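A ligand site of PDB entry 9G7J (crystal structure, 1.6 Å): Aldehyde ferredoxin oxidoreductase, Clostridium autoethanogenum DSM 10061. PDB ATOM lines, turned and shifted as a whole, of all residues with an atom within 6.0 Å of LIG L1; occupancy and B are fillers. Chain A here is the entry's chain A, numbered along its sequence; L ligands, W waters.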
ATOM      1  N   THR A  73     -24.661 -22.317 -19.655  1.00  0.00           N
ATOM      2  CA  THR A  73     -23.796 -23.491 -19.310  1.00  0.00           C
ATOM      3  C   THR A  73     -22.340 -23.291 -19.765  1.00  0.00           C
ATOM      4  O   THR A  73     -21.717 -24.298 -20.129  1.00  0.00           O
ATOM      5  CB  THR A  73     -24.421 -24.793 -19.821  1.00  0.00           C
ATOM      6  OG1 THR A  73     -24.198 -24.938 -21.224  1.00  0.00           O
ATOM      7  CG2 THR A  73     -25.905 -24.880 -19.517  1.00  0.00           C
ATOM      8  N   GLY A  75     -19.639 -22.820 -18.079  1.00  0.00           N
ATOM      9  CA  GLY A  75     -18.646 -23.047 -17.007  1.00  0.00           C
ATOM     10  C   GLY A  75     -17.863 -24.339 -17.213  1.00  0.00           C
ATOM     11  O   GLY A  75     -17.067 -24.658 -16.328  1.00  0.00           O
ATOM     12  N   ARG A  76     -18.038 -25.007 -18.352  1.00  0.00           N
ATOM     13  CA  ARG A  76     -17.420 -26.347 -18.549  1.00  0.00           C
ATOM     14  C   ARG A  76     -15.963 -26.280 -19.045  1.00  0.00           C
ATOM     15  O   ARG A  76     -15.657 -25.409 -19.868  1.00  0.00           O
ATOM     16  CB  ARG A  76     -18.249 -27.179 -19.527  1.00  0.00           C
ATOM     17  CG  ARG A  76     -19.718 -27.320 -19.140  1.00  0.00           C
ATOM     18  CD  ARG A  76     -19.945 -27.812 -17.724  1.00  0.00           C
ATOM     19  NE  ARG A  76     -19.426 -29.153 -17.507  1.00  0.00           N
ATOM     20  CZ  ARG A  76     -19.833 -29.979 -16.561  1.00  0.00           C
ATOM     21  NH1 ARG A  76     -20.879 -29.664 -15.810  1.00  0.00           N
ATOM     22  NH2 ARG A  76     -19.202 -31.118 -16.354  1.00  0.00           N
ATOM     23  N   GLY A  95     -17.549 -28.737 -14.233  1.00  0.00           N
ATOM     24  CA  GLY A  95     -18.219 -27.424 -14.315  1.00  0.00           C
ATOM     25  C   GLY A  95     -17.830 -26.570 -13.133  1.00  0.00           C
ATOM     26  O   GLY A  95     -16.635 -26.476 -12.845  1.00  0.00           O
ATOM     27  N   GLY A  96     -18.823 -25.975 -12.466  1.00  0.00           N
ATOM     28  CA  GLY A  96     -18.538 -25.079 -11.346  1.00  0.00           C
ATOM     29  C   GLY A  96     -18.102 -23.695 -11.807  1.00  0.00           C
ATOM     30  O   GLY A  96     -18.816 -23.105 -12.623  1.00  0.00           O
ATOM     31  N   ARG A 181     -17.149 -30.250  -7.380  1.00  0.00           N
ATOM     32  CA  ARG A 181     -17.285 -30.520  -8.831  1.00  0.00           C
ATOM     33  C   ARG A 181     -16.057 -31.342  -9.241  1.00  0.00           C
ATOM     34  O   ARG A 181     -15.058 -31.254  -8.565  1.00  0.00           O
ATOM     35  CB  ARG A 181     -17.465 -29.222  -9.618  1.00  0.00           C
ATOM     36  CG  ARG A 181     -18.553 -28.299  -9.097  1.00  0.00           C
ATOM     37  CD  ARG A 181     -19.922 -28.939  -8.967  1.00  0.00           C
ATOM     38  NE  ARG A 181     -20.502 -29.312 -10.253  1.00  0.00           N
ATOM     39  CZ  ARG A 181     -21.769 -29.630 -10.443  1.00  0.00           C
ATOM     40  NH1 ARG A 181     -22.633 -29.609  -9.435  1.00  0.00           N
ATOM     41  NH2 ARG A 181     -22.196 -29.954 -11.644  1.00  0.00           N
ATOM     42  N   MET A 237     -34.957 -30.988 -14.089  1.00  0.00           N
ATOM     43  CA  MET A 237     -33.548 -30.917 -13.601  1.00  0.00           C
ATOM     44  C   MET A 237     -33.432 -29.927 -12.427  1.00  0.00           C
ATOM     45  O   MET A 237     -32.703 -30.247 -11.471  1.00  0.00           O
ATOM     46  CB  MET A 237     -32.579 -30.521 -14.716  1.00  0.00           C
ATOM     47  CG  MET A 237     -32.639 -31.412 -15.932  1.00  0.00           C
ATOM     48  SD  MET A 237     -31.010 -32.066 -16.351  1.00  0.00           S
ATOM     49  CE  MET A 237     -30.819 -33.305 -15.076  1.00  0.00           C
ATOM     50  N   ASN A 285     -27.499 -25.897  -6.858  1.00  0.00           N
ATOM     51  CA  ASN A 285     -26.090 -25.435  -6.810  1.00  0.00           C
ATOM     52  C   ASN A 285     -25.648 -25.259  -8.261  1.00  0.00           C
ATOM     53  O   ASN A 285     -24.841 -26.073  -8.736  1.00  0.00           O
ATOM     54  CB  ASN A 285     -25.223 -26.440  -6.048  1.00  0.00           C
ATOM     55  CG  ASN A 285     -23.876 -25.861  -5.662  1.00  0.00           C
ATOM     56  OD1 ASN A 285     -23.769 -24.677  -5.363  1.00  0.00           O
ATOM     57  ND2 ASN A 285     -22.851 -26.698  -5.668  1.00  0.00           N
ATOM     58  N   PRO A 286     -26.181 -24.260  -8.988  1.00  0.00           N
ATOM     59  CA  PRO A 286     -25.897 -24.135 -10.418  1.00  0.00           C
ATOM     60  C   PRO A 286     -24.457 -23.767 -10.791  1.00  0.00           C
ATOM     61  O   PRO A 286     -23.853 -22.985 -10.096  1.00  0.00           O
ATOM     62  CB  PRO A 286     -26.851 -22.999 -10.866  1.00  0.00           C
ATOM     63  CG  PRO A 286     -27.870 -22.899  -9.758  1.00  0.00           C
ATOM     64  CD  PRO A 286     -27.095 -23.228  -8.498  1.00  0.00           C
ATOM     65  N   CYS A 287     -23.964 -24.361 -11.873  1.00  0.00           N
ATOM     66  CA  CYS A 287     -22.624 -23.979 -12.372  1.00  0.00           C
ATOM     67  C   CYS A 287     -22.701 -22.570 -12.971  1.00  0.00           C
ATOM     68  O   CYS A 287     -23.798 -21.998 -13.013  1.00  0.00           O
ATOM     69  CB  CYS A 287     -22.154 -24.897 -13.483  1.00  0.00           C
ATOM     70  SG  CYS A 287     -22.018 -26.649 -13.004  1.00  0.00           S
ATOM     71  N   TYR A 288     -21.576 -22.063 -13.451  1.00  0.00           N
ATOM     72  CA  TYR A 288     -21.513 -20.706 -14.040  1.00  0.00           C
ATOM     73  C   TYR A 288     -22.496 -20.511 -15.189  1.00  0.00           C
ATOM     74  O   TYR A 288     -22.583 -21.408 -16.042  1.00  0.00           O
ATOM     75  CB  TYR A 288     -20.095 -20.432 -14.539  1.00  0.00           C
ATOM     76  CG  TYR A 288     -19.836 -19.017 -14.998  1.00  0.00           C
ATOM     77  CD1 TYR A 288     -19.513 -18.025 -14.087  1.00  0.00           C
ATOM     78  CD2 TYR A 288     -19.924 -18.665 -16.333  1.00  0.00           C
ATOM     79  CE1 TYR A 288     -19.271 -16.724 -14.486  1.00  0.00           C
ATOM     80  CE2 TYR A 288     -19.685 -17.371 -16.748  1.00  0.00           C
ATOM     81  CZ  TYR A 288     -19.364 -16.397 -15.825  1.00  0.00           C
ATOM     82  OH  TYR A 288     -19.128 -15.107 -16.232  1.00  0.00           O
ATOM     83  N   CYS A 290     -25.574 -20.840 -15.712  1.00  0.00           N
ATOM     84  CA  CYS A 290     -26.459 -21.997 -16.001  1.00  0.00           C
ATOM     85  C   CYS A 290     -27.905 -21.728 -15.571  1.00  0.00           C
ATOM     86  O   CYS A 290     -28.139 -21.519 -14.377  1.00  0.00           O
ATOM     87  CB  CYS A 290     -25.957 -23.243 -15.296  1.00  0.00           C
ATOM     88  SG  CYS A 290     -27.011 -24.670 -15.685  1.00  0.00           S
ATOM     89  N   PRO A 291     -28.869 -21.732 -16.513  1.00  0.00           N
ATOM     90  CA  PRO A 291     -30.290 -21.570 -16.161  1.00  0.00           C
ATOM     91  C   PRO A 291     -30.954 -22.887 -15.745  1.00  0.00           C
ATOM     92  O   PRO A 291     -32.076 -22.850 -15.307  1.00  0.00           O
ATOM     93  CB  PRO A 291     -30.886 -21.083 -17.481  1.00  0.00           C
ATOM     94  CG  PRO A 291     -30.057 -21.770 -18.543  1.00  0.00           C
ATOM     95  CD  PRO A 291     -28.668 -21.859 -17.950  1.00  0.00           C
ATOM     96  N   ILE A 292     -30.239 -24.003 -15.883  1.00  0.00           N
ATOM     97  CA  ILE A 292     -30.827 -25.350 -15.566  1.00  0.00           C
ATOM     98  C   ILE A 292     -30.665 -25.629 -14.063  1.00  0.00           C
ATOM     99  O   ILE A 292     -31.669 -25.964 -13.437  1.00  0.00           O
ATOM    100  CB  ILE A 292     -30.177 -26.438 -16.443  1.00  0.00           C
ATOM    101  CG1 ILE A 292     -30.338 -26.127 -17.938  1.00  0.00           C
ATOM    102  CG2 ILE A 292     -30.734 -27.815 -16.108  1.00  0.00           C
ATOM    103  CD1 ILE A 292     -29.598 -27.067 -18.853  1.00  0.00           C
ATOM    104  N   GLY A 293     -29.454 -25.487 -13.522  1.00  0.00           N
ATOM    105  CA  GLY A 293     -29.252 -25.623 -12.067  1.00  0.00           C
ATOM    106  C   GLY A 293     -29.549 -27.030 -11.556  1.00  0.00           C
ATOM    107  O   GLY A 293     -30.215 -27.146 -10.530  1.00  0.00           O
ATOM    108  N   CYS A 294     -29.035 -28.041 -12.254  1.00  0.00           N
ATOM    109  CA  CYS A 294     -29.257 -29.450 -11.828  1.00  0.00           C
ATOM    110  C   CYS A 294     -28.402 -29.738 -10.587  1.00  0.00           C
ATOM    111  O   CYS A 294     -28.711 -30.695  -9.863  1.00  0.00           O
ATOM    112  CB  CYS A 294     -28.965 -30.429 -12.966  1.00  0.00           C
ATOM    113  SG  CYS A 294     -27.213 -30.845 -13.200  1.00  0.00           S
ATOM    114  N   GLY A 295     -27.412 -28.891 -10.319  1.00  0.00           N
ATOM    115  CA  GLY A 295     -26.519 -29.102  -9.165  1.00  0.00           C
ATOM    116  C   GLY A 295     -27.291 -29.228  -7.868  1.00  0.00           C
ATOM    117  O   GLY A 295     -28.279 -28.516  -7.702  1.00  0.00           O
ATOM    118  N   GLU A 310     -25.295 -37.058  -7.643  1.00  0.00           N
ATOM    119  CA  GLU A 310     -25.920 -37.136  -8.979  1.00  0.00           C
ATOM    120  C   GLU A 310     -26.544 -38.527  -9.127  1.00  0.00           C
ATOM    121  O   GLU A 310     -26.309 -39.381  -8.265  1.00  0.00           O
ATOM    122  CB  GLU A 310     -24.868 -36.970 -10.077  1.00  0.00           C
ATOM    123  CG  GLU A 310     -23.959 -35.775  -9.854  1.00  0.00           C
ATOM    124  CD  GLU A 310     -24.588 -34.455 -10.233  1.00  0.00           C
ATOM    125  OE1 GLU A 310     -25.746 -34.466 -10.702  1.00  0.00           O
ATOM    126  OE2 GLU A 310     -23.924 -33.415 -10.070  1.00  0.00           O
ATOM    127  N   CYS A 493     -22.439 -27.339 -21.553  1.00  0.00           N
ATOM    128  CA  CYS A 493     -22.911 -28.548 -20.832  1.00  0.00           C
ATOM    129  C   CYS A 493     -23.748 -29.447 -21.743  1.00  0.00           C
ATOM    130  O   CYS A 493     -24.589 -28.918 -22.483  1.00  0.00           O
ATOM    131  CB  CYS A 493     -23.735 -28.132 -19.624  1.00  0.00           C
ATOM    132  SG  CYS A 493     -24.324 -29.531 -18.632  1.00  0.00           S
ATOM    133  N   ILE A 494     -23.544 -30.753 -21.658  1.00  0.00           N
ATOM    134  CA  ILE A 494     -24.298 -31.731 -22.500  1.00  0.00           C
ATOM    135  C   ILE A 494     -25.799 -31.617 -22.218  1.00  0.00           C
ATOM    136  O   ILE A 494     -26.586 -31.983 -23.101  1.00  0.00           O
ATOM    137  CB  ILE A 494     -23.770 -33.155 -22.243  1.00  0.00           C
ATOM    138  CG1 ILE A 494     -24.258 -34.136 -23.306  1.00  0.00           C
ATOM    139  CG2 ILE A 494     -24.110 -33.618 -20.839  1.00  0.00           C
ATOM    140  CD1 ILE A 494     -23.829 -33.788 -24.708  1.00  0.00           C
ATOM    141  N   PHE A 495     -26.182 -31.122 -21.045  1.00  0.00           N
ATOM    142  CA  PHE A 495     -27.622 -31.081 -20.674  1.00  0.00           C
ATOM    143  C   PHE A 495     -28.350 -30.001 -21.474  1.00  0.00           C
ATOM    144  O   PHE A 495     -29.577 -29.902 -21.356  1.00  0.00           O
ATOM    145  CB  PHE A 495     -27.800 -30.921 -19.159  1.00  0.00           C
ATOM    146  CG  PHE A 495     -27.357 -32.120 -18.351  1.00  0.00           C
ATOM    147  CD1 PHE A 495     -27.458 -33.396 -18.884  1.00  0.00           C
ATOM    148  CD2 PHE A 495     -26.837 -31.972 -17.086  1.00  0.00           C
ATOM    149  CE1 PHE A 495     -27.053 -34.496 -18.154  1.00  0.00           C
ATOM    150  CE2 PHE A 495     -26.420 -33.079 -16.355  1.00  0.00           C
ATOM    151  CZ  PHE A 495     -26.533 -34.335 -16.893  1.00  0.00           C
HETATM  152 FE1  LIG L   1     -24.832 -28.660 -16.467  1.00  0.00          FE
HETATM  153 FE2  LIG L   1     -26.094 -29.027 -14.176  1.00  0.00          FE
HETATM  154 FE3  LIG L   1     -25.952 -26.584 -15.254  1.00  0.00          FE
HETATM  155 FE4  LIG L   1     -23.842 -27.672 -14.181  1.00  0.00          FE
HETATM  156  S1  LIG L   1     -25.732 -27.051 -13.000  1.00  0.00           S
HETATM  157  S2  LIG L   1     -23.849 -26.582 -16.220  1.00  0.00           S
HETATM  158  S3  LIG L   1     -24.038 -29.925 -14.704  1.00  0.00           S
HETATM  159  S4  LIG L   1     -27.090 -28.392 -16.153  1.00  0.00           S
HETATM  160  C1  LG2 L   2     -18.617 -37.709 -15.164  1.00  0.00           C
HETATM  161  C2  LG2 L   2     -19.109 -38.632 -14.051  1.00  0.00           C
HETATM  162  C3  LG2 L   2     -20.573 -38.407 -13.775  1.00  0.00           C
HETATM  163  S1  LG2 L   2     -21.588 -38.077 -15.075  1.00  0.00           S
HETATM  164  C4  LG2 L   2     -21.078 -38.465 -12.546  1.00  0.00           C
HETATM  165  S2  LG2 L   2     -22.728 -38.362 -12.325  1.00  0.00           S
HETATM  166  C5  LG2 L   2     -20.203 -38.632 -11.348  1.00  0.00           C
HETATM  167  N1  LG2 L   2     -20.028 -37.382 -10.632  1.00  0.00           N
HETATM  168  C6  LG2 L   2     -19.164 -37.407  -9.611  1.00  0.00           C
HETATM  169  C7  LG2 L   2     -19.297 -36.562  -8.419  1.00  0.00           C
HETATM  170  O1  LG2 L   2     -20.227 -35.750  -8.319  1.00  0.00           O
HETATM  171  N2  LG2 L   2     -18.376 -36.678  -7.454  1.00  0.00           N
HETATM  172  C8  LG2 L   2     -17.356 -37.560  -7.550  1.00  0.00           C
HETATM  173  N3  LG2 L   2     -16.465 -37.626  -6.542  1.00  0.00           N
HETATM  174  N4  LG2 L   2     -17.188 -38.363  -8.619  1.00  0.00           N
HETATM  175  C9  LG2 L   2     -18.030 -38.344  -9.660  1.00  0.00           C
HETATM  176  N5  LG2 L   2     -17.874 -39.154 -10.725  1.00  0.00           N
HETATM  177  C10 LG2 L   2     -18.844 -39.163 -11.794  1.00  0.00           C
HETATM  178  O2  LG2 L   2     -18.375 -38.352 -12.861  1.00  0.00           O
HETATM  179  C11 LG2 L   2     -21.464 -33.281 -13.505  1.00  0.00           C
HETATM  180  C12 LG2 L   2     -22.514 -33.115 -14.597  1.00  0.00           C
HETATM  181  C13 LG2 L   2     -23.099 -34.463 -14.914  1.00  0.00           C
HETATM  182  S3  LG2 L   2     -23.720 -35.387 -13.653  1.00  0.00           S
HETATM  183  C14 LG2 L   2     -23.159 -34.931 -16.161  1.00  0.00           C
HETATM  184  S4  LG2 L   2     -23.875 -36.438 -16.424  1.00  0.00           S
HETATM  185  C15 LG2 L   2     -22.666 -34.128 -17.321  1.00  0.00           C
HETATM  186  N6  LG2 L   2     -21.307 -34.409 -17.753  1.00  0.00           N
HETATM  187  C16 LG2 L   2     -20.927 -33.654 -18.800  1.00  0.00           C
HETATM  188  C17 LG2 L   2     -20.037 -34.117 -19.890  1.00  0.00           C
HETATM  189  O3  LG2 L   2     -19.554 -35.261 -19.863  1.00  0.00           O
HETATM  190  N7  LG2 L   2     -19.759 -33.266 -20.881  1.00  0.00           N
HETATM  191  C18 LG2 L   2     -20.264 -32.018 -20.928  1.00  0.00           C
HETATM  192  N8  LG2 L   2     -19.943 -31.210 -21.966  1.00  0.00           N
HETATM  193  N9  LG2 L   2     -21.094 -31.529 -19.971  1.00  0.00           N
HETATM  194  C19 LG2 L   2     -21.456 -32.280 -18.916  1.00  0.00           C
HETATM  195  N10 LG2 L   2     -22.283 -31.800 -17.963  1.00  0.00           N
HETATM  196  C20 LG2 L   2     -22.741 -32.664 -16.899  1.00  0.00           C
HETATM  197  O4  LG2 L   2     -21.911 -32.536 -15.752  1.00  0.00           O
HETATM  198  P1  LG2 L   2     -16.187 -36.994 -15.882  1.00  0.00           P
HETATM  199  O5  LG2 L   2     -16.149 -35.953 -14.658  1.00  0.00           O
HETATM  200  O6  LG2 L   2     -14.856 -37.678 -15.953  1.00  0.00           O
HETATM  201  O7  LG2 L   2     -16.545 -36.262 -17.141  1.00  0.00           O
HETATM  202  O8  LG2 L   2     -17.311 -38.098 -15.558  1.00  0.00           O
HETATM  203  P2  LG2 L   2     -19.317 -31.986 -12.780  1.00  0.00           P
HETATM  204  O9  LG2 L   2     -18.440 -32.569 -13.982  1.00  0.00           O
HETATM  205  O10 LG2 L   2     -18.938 -30.563 -12.509  1.00  0.00           O
HETATM  206  O11 LG2 L   2     -19.135 -32.865 -11.563  1.00  0.00           O
HETATM  207  O12 LG2 L   2     -20.864 -32.026 -13.227  1.00  0.00           O
HETATM  208 MG1  LG2 L   2     -17.241 -34.271 -14.276  1.00  0.00          MG
HETATM  209  W1  LG2 L   2     -23.985 -37.700 -14.261  1.00  0.00           W
HETATM  210  O   HOH W   1     -21.788 -23.926 -16.685  1.00  0.00           O
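N of Cys 294 lies close to S1 of LIG L1, 3.5 Å away. The side-chain sulfur (SG) of Cys 493 lies close to a nitrogen (N10) of LG2 L2 (3.1 Å). The guanidinium group (NH1) of Arg 76 lies close to a sulfur (S3) of LIG L1 (3.4 Å). The guanidinium group (NH2) of Arg 181 lies close to a sulfur (S3) of LIG L1. The backbone NH of Ile 494 lies within hydrogen-bond range of a nitrogen (N9) of LG2 L2 (3.1 Å). N of Cys 287 lies close to S1 of LIG L1. The backbone NH (N) of Gly 295 lies close to a sulfur (S1) of LIG L1 (3.7 Å). NE of Arg 181 lies within salt-bridge range of O10 of LG2 L2 (3.0 Å). O10 of LG2 L2 lies within hydrogen-bond range of N of Gly 95, at 2.9 Å. An iron atom (FE3) of LIG L1 is bound by the side-chain sulfur (SG) of Cys 290, at 2.2 Å. The side-chain sulfur (SG) of Cys 294 binds an iron atom (FE2) of LIG L1 (2.3 Å). An oxygen (O10) of LG2 L2 lies within salt-bridge range of the guanidinium group (NH2) of Arg 76 (3.9 Å). SG of Cys 287 binds FE4 of LIG L1, at 2.4 Å. FE1 of LIG L1 is bound by SG of Cys 493.
SG of Cys 287 sits close to NH2 of Arg 181 (3.6 Å). The backbone NH of Gly 96 sits close to the side-chain sulfur of Cys 287 (3.3 Å). N of Cys 493 sits at hydrogen-bond distance from OG1 of Thr 73 (3.0 Å). The backbone NH of Ile 292 lies close to the side-chain sulfur of Cys 290, 3.3 Å away. The backbone carbonyl oxygen of Gly 295 lies within hydrogen-bond range of the backbone NH of Asn 285. The backbone NH of Phe 495 lies close to the side-chain sulfur of Cys 493 (3.4 Å). N of Gly 293 sits close to SG of Cys 290 (3.4 Å).
Pro 286 touches LIG L1 (CA to S1, 3.9 Å). Ile 292 touches LIG L1. Gly 293 touches LIG L1. CD2 of Phe 495 touches S4 of LIG L1, 3.7 Å away. Hydrophobic or aromatic side chains within 4 Å of LIG L1: Ile 292 and Phe 495. 11 residues have an atom within 4 Å of LIG L1: Arg 76, Arg 181, Pro 286, Cys 287, Cys 290, Ile 292, Gly 293, Cys 294, Gly 295, Cys 493 and Phe 495.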
